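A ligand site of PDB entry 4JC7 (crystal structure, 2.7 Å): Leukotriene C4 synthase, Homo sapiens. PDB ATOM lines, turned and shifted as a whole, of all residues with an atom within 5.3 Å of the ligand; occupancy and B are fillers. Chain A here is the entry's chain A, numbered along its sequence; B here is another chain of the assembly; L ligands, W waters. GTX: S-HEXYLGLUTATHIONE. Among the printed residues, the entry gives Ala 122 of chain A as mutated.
Residues that only touch the ligand: Asn 61, Leu 114, Ile 33 of chain B, Ala 118, Tyr 65, Tyr 56 of chain B, Ala 122, Val 32 of chain B and Leu 30 of chain B.
Hydrophobic or aromatic side chains that line the ligand: Tyr 65, Tyr 99, Leu 114, Ala 122, Leu 30 of chain B, Val 32 of chain B, Ile 33 of chain B and Tyr 56 of chain B.
A nitrogen (N1) of the ligand is in salt-bridge range of the side-chain carboxylate (OE1) of Glu 64 (3.0 Å).
The side-chain hydroxyl (OH) of Tyr 99 is in hydrogen-bond range of an oxygen (O31) of the ligand.
The guanidinium group (NH2) of Arg 36 of chain B lies within salt-bridge range of an oxygen (O12) of the ligand (2.9 Å).
A nitrogen (N1) of the ligand lies close to the side-chain amide oxygen of Gln 59 of chain B (3.2 Å).
The side-chain hydroxyl (OG) of Ser 29 of chain B sits at hydrogen-bond distance from an oxygen (OE1) of the ligand (3.3 Å).
NE of Arg 110 is in salt-bridge range of O31 of the ligand (3.0 Å).
The side-chain hydroxyl (OH) of Tyr 99 sits at hydrogen-bond distance from the side-chain amide nitrogen (ND2) of Asn 61 (2.8 Å).
NH1 of Arg 57 is in hydrogen-bond range of OH of Tyr 56 of chain B, 3.4 Å away.
The side-chain carboxylate (OE2) of Glu 64 sits at hydrogen-bond distance from the side-chain amide nitrogen (NE2) of Gln 59 of chain B, 3.0 Å away.
OH of Tyr 65 is in hydrogen-bond range of OG of Ser 29 of chain B (2.8 Å).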
ATOM      1  N   ARG A  57      25.305  12.631  31.448  1.00  0.00           N
ATOM      2  CA  ARG A  57      24.432  13.406  30.638  1.00  0.00           C
ATOM      3  C   ARG A  57      23.930  12.542  29.485  1.00  0.00           C
ATOM      4  O   ARG A  57      22.793  12.724  29.009  1.00  0.00           O
ATOM      5  CB  ARG A  57      25.127  14.668  30.145  1.00  0.00           C
ATOM      6  CG  ARG A  57      24.334  15.506  29.224  1.00  0.00           C
ATOM      7  CD  ARG A  57      23.222  16.231  29.949  1.00  0.00           C
ATOM      8  NE  ARG A  57      23.532  16.585  31.334  1.00  0.00           N
ATOM      9  CZ  ARG A  57      22.613  16.605  32.302  1.00  0.00           C
ATOM     10  NH1 ARG A  57      21.359  16.328  31.988  1.00  0.00           N
ATOM     11  NH2 ARG A  57      22.927  16.921  33.557  1.00  0.00           N
ATOM     12  N   ASN A  61      19.985  11.922  28.757  1.00  0.00           N
ATOM     13  CA  ASN A  61      19.288  12.266  27.513  1.00  0.00           C
ATOM     14  C   ASN A  61      18.566  11.052  26.961  1.00  0.00           C
ATOM     15  O   ASN A  61      17.406  11.130  26.545  1.00  0.00           O
ATOM     16  CB  ASN A  61      20.229  12.855  26.446  1.00  0.00           C
ATOM     17  CG  ASN A  61      20.695  14.255  26.785  1.00  0.00           C
ATOM     18  OD1 ASN A  61      20.048  14.987  27.547  1.00  0.00           O
ATOM     19  ND2 ASN A  61      21.796  14.675  26.170  1.00  0.00           N
ATOM     20  N   GLU A  64      15.390  10.551  28.898  1.00  0.00           N
ATOM     21  CA  GLU A  64      14.372  11.498  28.544  1.00  0.00           C
ATOM     22  C   GLU A  64      13.713  11.080  27.194  1.00  0.00           C
ATOM     23  O   GLU A  64      12.488  11.180  27.028  1.00  0.00           O
ATOM     24  CB  GLU A  64      14.994  12.885  28.543  1.00  0.00           C
ATOM     25  CG  GLU A  64      14.413  13.963  27.711  1.00  0.00           C
ATOM     26  CD  GLU A  64      15.367  15.166  27.613  1.00  0.00           C
ATOM     27  OE1 GLU A  64      16.279  15.259  28.472  1.00  0.00           O
ATOM     28  OE2 GLU A  64      15.231  15.966  26.648  1.00  0.00           O
ATOM     29  N   TYR A  65      14.482  10.586  26.228  1.00  0.00           N
ATOM     30  CA  TYR A  65      13.866  10.206  24.954  1.00  0.00           C
ATOM     31  C   TYR A  65      13.203   8.815  24.941  1.00  0.00           C
ATOM     32  O   TYR A  65      12.445   8.533  24.038  1.00  0.00           O
ATOM     33  CB  TYR A  65      14.882  10.297  23.824  1.00  0.00           C
ATOM     34  CG  TYR A  65      14.861  11.674  23.273  1.00  0.00           C
ATOM     35  CD1 TYR A  65      14.021  11.948  22.208  1.00  0.00           C
ATOM     36  CD2 TYR A  65      15.542  12.730  23.858  1.00  0.00           C
ATOM     37  CE1 TYR A  65      13.884  13.210  21.691  1.00  0.00           C
ATOM     38  CE2 TYR A  65      15.437  14.024  23.337  1.00  0.00           C
ATOM     39  CZ  TYR A  65      14.587  14.240  22.248  1.00  0.00           C
ATOM     40  OH  TYR A  65      14.451  15.481  21.673  1.00  0.00           O
ATOM     41  N   ARG A  96      21.242   5.006  19.398  1.00  0.00           N
ATOM     42  CA  ARG A  96      21.372   5.415  20.788  1.00  0.00           C
ATOM     43  C   ARG A  96      22.549   4.799  21.546  1.00  0.00           C
ATOM     44  O   ARG A  96      23.171   5.489  22.372  1.00  0.00           O
ATOM     45  CB  ARG A  96      20.049   5.197  21.549  1.00  0.00           C
ATOM     46  CG  ARG A  96      19.005   6.226  21.212  1.00  0.00           C
ATOM     47  CD  ARG A  96      19.457   7.515  21.841  1.00  0.00           C
ATOM     48  NE  ARG A  96      18.532   8.608  21.644  1.00  0.00           N
ATOM     49  CZ  ARG A  96      18.658   9.778  22.250  1.00  0.00           C
ATOM     50  NH1 ARG A  96      19.632   9.934  23.137  1.00  0.00           N
ATOM     51  NH2 ARG A  96      17.788  10.766  22.017  1.00  0.00           N
ATOM     52  N   TYR A  99      25.373   6.786  20.238  1.00  0.00           N
ATOM     53  CA  TYR A  99      25.288   8.103  20.859  1.00  0.00           C
ATOM     54  C   TYR A  99      25.949   8.047  22.241  1.00  0.00           C
ATOM     55  O   TYR A  99      26.777   8.877  22.580  1.00  0.00           O
ATOM     56  CB  TYR A  99      23.826   8.561  20.931  1.00  0.00           C
ATOM     57  CG  TYR A  99      23.565   9.765  21.802  1.00  0.00           C
ATOM     58  CD1 TYR A  99      23.646  11.058  21.267  1.00  0.00           C
ATOM     59  CD2 TYR A  99      23.274   9.644  23.150  1.00  0.00           C
ATOM     60  CE1 TYR A  99      23.435  12.183  22.038  1.00  0.00           C
ATOM     61  CE2 TYR A  99      23.050  10.764  23.923  1.00  0.00           C
ATOM     62  CZ  TYR A  99      23.150  12.023  23.364  1.00  0.00           C
ATOM     63  OH  TYR A  99      22.892  13.097  24.138  1.00  0.00           O
ATOM     64  N   TYR A 103      29.384  10.007  23.174  1.00  0.00           N
ATOM     65  CA  TYR A 103      29.339  11.025  24.207  1.00  0.00           C
ATOM     66  C   TYR A 103      30.342  10.715  25.311  1.00  0.00           C
ATOM     67  O   TYR A 103      31.033  11.621  25.790  1.00  0.00           O
ATOM     68  CB  TYR A 103      27.934  11.107  24.786  1.00  0.00           C
ATOM     69  CG  TYR A 103      27.571  12.458  25.320  1.00  0.00           C
ATOM     70  CD1 TYR A 103      28.532  13.415  25.573  1.00  0.00           C
ATOM     71  CD2 TYR A 103      26.241  12.778  25.550  1.00  0.00           C
ATOM     72  CE1 TYR A 103      28.190  14.660  26.045  1.00  0.00           C
ATOM     73  CE2 TYR A 103      25.889  14.030  26.027  1.00  0.00           C
ATOM     74  CZ  TYR A 103      26.858  14.966  26.271  1.00  0.00           C
ATOM     75  OH  TYR A 103      26.499  16.203  26.758  1.00  0.00           O
ATOM     76  N   ARG A 110      29.268  12.294  20.123  1.00  0.00           N
ATOM     77  CA  ARG A 110      27.892  11.944  20.370  1.00  0.00           C
ATOM     78  C   ARG A 110      27.058  12.392  19.141  1.00  0.00           C
ATOM     79  O   ARG A 110      25.975  11.855  18.887  1.00  0.00           O
ATOM     80  CB  ARG A 110      27.346  12.590  21.644  1.00  0.00           C
ATOM     81  CG  ARG A 110      26.676  13.930  21.383  1.00  0.00           C
ATOM     82  CD  ARG A 110      26.401  14.672  22.665  1.00  0.00           C
ATOM     83  NE  ARG A 110      25.570  15.841  22.432  1.00  0.00           N
ATOM     84  CZ  ARG A 110      26.010  16.983  21.924  1.00  0.00           C
ATOM     85  NH1 ARG A 110      25.204  18.025  21.748  1.00  0.00           N
ATOM     86  NH2 ARG A 110      27.299  17.076  21.590  1.00  0.00           N
ATOM     87  N   LEU A 114      23.594  10.669  17.387  1.00  0.00           N
ATOM     88  CA  LEU A 114      22.440  11.491  17.707  1.00  0.00           C
ATOM     89  C   LEU A 114      21.542  11.777  16.511  1.00  0.00           C
ATOM     90  O   LEU A 114      20.335  11.610  16.559  1.00  0.00           O
ATOM     91  CB  LEU A 114      22.815  12.798  18.399  1.00  0.00           C
ATOM     92  CG  LEU A 114      21.610  13.694  18.703  1.00  0.00           C
ATOM     93  CD1 LEU A 114      20.640  12.989  19.649  1.00  0.00           C
ATOM     94  CD2 LEU A 114      22.022  15.072  19.178  1.00  0.00           C
ATOM     95  N   ALA A 118      17.707  10.548  15.721  1.00  0.00           N
ATOM     96  CA  ALA A 118      16.608  11.470  15.479  1.00  0.00           C
ATOM     97  C   ALA A 118      15.867  11.147  14.168  1.00  0.00           C
ATOM     98  O   ALA A 118      14.671  11.380  14.066  1.00  0.00           O
ATOM     99  CB  ALA A 118      17.068  12.913  15.497  1.00  0.00           C
ATOM    100  N   LEU A 121      13.615   8.130  14.735  1.00  0.00           N
ATOM    101  CA  LEU A 121      12.504   8.579  15.535  1.00  0.00           C
ATOM    102  C   LEU A 121      11.499   9.367  14.714  1.00  0.00           C
ATOM    103  O   LEU A 121      10.285   9.254  14.917  1.00  0.00           O
ATOM    104  CB  LEU A 121      12.970   9.366  16.743  1.00  0.00           C
ATOM    105  CG  LEU A 121      11.870   9.711  17.715  1.00  0.00           C
ATOM    106  CD1 LEU A 121      11.147   8.457  18.201  1.00  0.00           C
ATOM    107  CD2 LEU A 121      12.510  10.394  18.889  1.00  0.00           C
ATOM    108  N   ALA A 122      12.018  10.215  13.830  1.00  0.00           N
ATOM    109  CA  ALA A 122      11.162  11.007  12.977  1.00  0.00           C
ATOM    110  C   ALA A 122      10.407  10.149  11.968  1.00  0.00           C
ATOM    111  O   ALA A 122       9.257  10.422  11.623  1.00  0.00           O
ATOM    112  CB  ALA A 122      11.961  12.047  12.277  1.00  0.00           C
ATOM    113  N   ALA B  26       8.854  16.918  21.666  1.00  0.00           N
ATOM    114  CA  ALA B  26       9.865  17.154  20.658  1.00  0.00           C
ATOM    115  C   ALA B  26      10.048  18.649  20.493  1.00  0.00           C
ATOM    116  O   ALA B  26      11.183  19.174  20.395  1.00  0.00           O
ATOM    117  CB  ALA B  26       9.454  16.543  19.348  1.00  0.00           C
ATOM    118  N   SER B  29      12.041  20.007  23.199  1.00  0.00           N
ATOM    119  CA  SER B  29      13.445  19.705  22.990  1.00  0.00           C
ATOM    120  C   SER B  29      14.139  20.677  22.025  1.00  0.00           C
ATOM    121  O   SER B  29      15.285  21.122  22.272  1.00  0.00           O
ATOM    122  CB  SER B  29      13.610  18.280  22.479  1.00  0.00           C
ATOM    123  OG  SER B  29      13.628  17.363  23.561  1.00  0.00           O
ATOM    124  N   LEU B  30      13.447  20.993  20.929  1.00  0.00           N
ATOM    125  CA  LEU B  30      14.011  21.946  19.985  1.00  0.00           C
ATOM    126  C   LEU B  30      14.107  23.317  20.664  1.00  0.00           C
ATOM    127  O   LEU B  30      15.072  24.052  20.418  1.00  0.00           O
ATOM    128  CB  LEU B  30      13.198  22.038  18.682  1.00  0.00           C
ATOM    129  CG  LEU B  30      13.076  20.847  17.737  1.00  0.00           C
ATOM    130  CD1 LEU B  30      12.041  21.120  16.674  1.00  0.00           C
ATOM    131  CD2 LEU B  30      14.418  20.547  17.095  1.00  0.00           C
ATOM    132  N   VAL B  32      14.781  23.844  23.870  1.00  0.00           N
ATOM    133  CA  VAL B  32      15.969  23.812  24.696  1.00  0.00           C
ATOM    134  C   VAL B  32      17.222  23.963  23.851  1.00  0.00           C
ATOM    135  O   VAL B  32      18.129  24.665  24.242  1.00  0.00           O
ATOM    136  CB  VAL B  32      16.038  22.544  25.563  1.00  0.00           C
ATOM    137  CG1 VAL B  32      17.377  22.453  26.289  1.00  0.00           C
ATOM    138  CG2 VAL B  32      14.926  22.581  26.545  1.00  0.00           C
ATOM    139  N   ILE B  33      17.304  23.285  22.709  1.00  0.00           N
ATOM    140  CA  ILE B  33      18.490  23.463  21.862  1.00  0.00           C
ATOM    141  C   ILE B  33      18.637  24.926  21.372  1.00  0.00           C
ATOM    142  O   ILE B  33      19.751  25.495  21.315  1.00  0.00           O
ATOM    143  CB  ILE B  33      18.463  22.508  20.689  1.00  0.00           C
ATOM    144  CG1 ILE B  33      18.963  21.191  21.233  1.00  0.00           C
ATOM    145  CG2 ILE B  33      19.521  22.828  19.670  1.00  0.00           C
ATOM    146  CD1 ILE B  33      18.761  20.102  20.322  1.00  0.00           C
ATOM    147  N   ARG B  36      19.978  26.895  24.124  1.00  0.00           N
ATOM    148  CA  ARG B  36      21.408  26.584  24.158  1.00  0.00           C
ATOM    149  C   ARG B  36      22.225  27.423  23.160  1.00  0.00           C
ATOM    150  O   ARG B  36      23.347  27.840  23.468  1.00  0.00           O
ATOM    151  CB  ARG B  36      21.688  25.102  23.872  1.00  0.00           C
ATOM    152  CG  ARG B  36      21.745  24.226  25.122  1.00  0.00           C
ATOM    153  CD  ARG B  36      22.071  22.781  24.783  1.00  0.00           C
ATOM    154  NE  ARG B  36      21.866  21.872  25.906  1.00  0.00           N
ATOM    155  CZ  ARG B  36      22.620  21.822  26.999  1.00  0.00           C
ATOM    156  NH1 ARG B  36      23.661  22.646  27.143  1.00  0.00           N
ATOM    157  NH2 ARG B  36      22.340  20.957  27.969  1.00  0.00           N
ATOM    158  N   PRO B  43      26.590  21.544  25.653  1.00  0.00           N
ATOM    159  CA  PRO B  43      26.590  20.253  26.361  1.00  0.00           C
ATOM    160  C   PRO B  43      27.984  19.741  26.751  1.00  0.00           C
ATOM    161  O   PRO B  43      28.929  19.948  25.989  1.00  0.00           O
ATOM    162  CB  PRO B  43      25.965  19.307  25.338  1.00  0.00           C
ATOM    163  CG  PRO B  43      25.143  20.177  24.476  1.00  0.00           C
ATOM    164  CD  PRO B  43      25.917  21.443  24.354  1.00  0.00           C
ATOM    165  N   THR B  46      24.206  22.362  32.445  1.00  0.00           N
ATOM    166  CA  THR B  46      22.792  22.643  32.324  1.00  0.00           C
ATOM    167  C   THR B  46      22.497  23.869  33.189  1.00  0.00           C
ATOM    168  O   THR B  46      21.348  24.153  33.580  1.00  0.00           O
ATOM    169  CB  THR B  46      22.027  21.400  32.822  1.00  0.00           C
ATOM    170  OG1 THR B  46      22.496  21.029  34.127  1.00  0.00           O
ATOM    171  CG2 THR B  46      22.238  20.222  31.847  1.00  0.00           C
ATOM    172  N   TYR B  56      15.152  25.115  30.190  1.00  0.00           N
ATOM    173  CA  TYR B  56      15.694  23.807  30.476  1.00  0.00           C
ATOM    174  C   TYR B  56      14.880  23.037  31.491  1.00  0.00           C
ATOM    175  O   TYR B  56      14.565  21.837  31.341  1.00  0.00           O
ATOM    176  CB  TYR B  56      17.149  23.912  30.942  1.00  0.00           C
ATOM    177  CG  TYR B  56      17.749  22.610  31.371  1.00  0.00           C
ATOM    178  CD1 TYR B  56      18.143  21.665  30.428  1.00  0.00           C
ATOM    179  CD2 TYR B  56      17.819  22.273  32.716  1.00  0.00           C
ATOM    180  CE1 TYR B  56      18.654  20.466  30.819  1.00  0.00           C
ATOM    181  CE2 TYR B  56      18.332  21.088  33.112  1.00  0.00           C
ATOM    182  CZ  TYR B  56      18.748  20.178  32.161  1.00  0.00           C
ATOM    183  OH  TYR B  56      19.283  18.964  32.565  1.00  0.00           O
ATOM    184  N   GLN B  59      11.403  22.014  30.274  1.00  0.00           N
ATOM    185  CA  GLN B  59      11.488  20.801  29.447  1.00  0.00           C
ATOM    186  C   GLN B  59      11.678  19.564  30.332  1.00  0.00           C
ATOM    187  O   GLN B  59      10.983  18.569  30.168  1.00  0.00           O
ATOM    188  CB  GLN B  59      12.580  20.949  28.409  1.00  0.00           C
ATOM    189  CG  GLN B  59      12.872  19.746  27.541  1.00  0.00           C
ATOM    190  CD  GLN B  59      13.986  18.910  28.120  1.00  0.00           C
ATOM    191  OE1 GLN B  59      15.144  19.368  28.183  1.00  0.00           O
ATOM    192  NE2 GLN B  59      13.677  17.686  28.540  1.00  0.00           N
HETATM  193  N1  GTX L   1      17.804  17.706  27.842  1.00  0.00           N
HETATM  194  CA1 GTX L   1      18.231  18.200  26.563  1.00  0.00           C
HETATM  195  C1  GTX L   1      19.476  19.049  26.691  1.00  0.00           C
HETATM  196  O11 GTX L   1      20.102  19.402  25.639  1.00  0.00           O
HETATM  197  O12 GTX L   1      19.903  19.423  27.830  1.00  0.00           O
HETATM  198  CB1 GTX L   1      17.070  18.923  25.965  1.00  0.00           C
HETATM  199  CG1 GTX L   1      16.984  19.205  24.510  1.00  0.00           C
HETATM  200  CD1 GTX L   1      17.049  18.011  23.658  1.00  0.00           C
HETATM  201  OE1 GTX L   1      16.818  16.922  24.158  1.00  0.00           O
HETATM  202  N2  GTX L   1      17.386  18.066  22.273  1.00  0.00           N
HETATM  203  CA2 GTX L   1      17.445  16.827  21.554  1.00  0.00           C
HETATM  204  C2  GTX L   1      18.693  16.124  21.973  1.00  0.00           C
HETATM  205  O2  GTX L   1      19.133  15.189  21.299  1.00  0.00           O
HETATM  206  CB2 GTX L   1      17.451  16.976  20.062  1.00  0.00           C
HETATM  207  SG2 GTX L   1      16.425  18.165  19.241  1.00  0.00           S
HETATM  208  C1S GTX L   1      14.814  17.506  18.955  1.00  0.00           C
HETATM  209  C2S GTX L   1      14.692  16.132  18.404  1.00  0.00           C
HETATM  210  C3S GTX L   1      13.292  15.634  18.326  1.00  0.00           C
HETATM  211  C4S GTX L   1      13.042  14.379  17.582  1.00  0.00           C
HETATM  212  C5S GTX L   1      12.260  14.462  16.311  1.00  0.00           C
HETATM  213  C6S GTX L   1      12.417  13.265  15.436  1.00  0.00           C
HETATM  214  N3  GTX L   1      19.381  16.561  23.162  1.00  0.00           N
HETATM  215  CA3 GTX L   1      20.576  15.916  23.598  1.00  0.00           C
HETATM  216  C3  GTX L   1      21.776  16.128  22.733  1.00  0.00           C
HETATM  217  O31 GTX L   1      22.608  15.193  22.575  1.00  0.00           O
HETATM  218  O32 GTX L   1      21.883  17.245  22.167  1.00  0.00           O
HETATM  219  O   HOH W   1      16.663  13.605  19.656  1.00  0.00           O
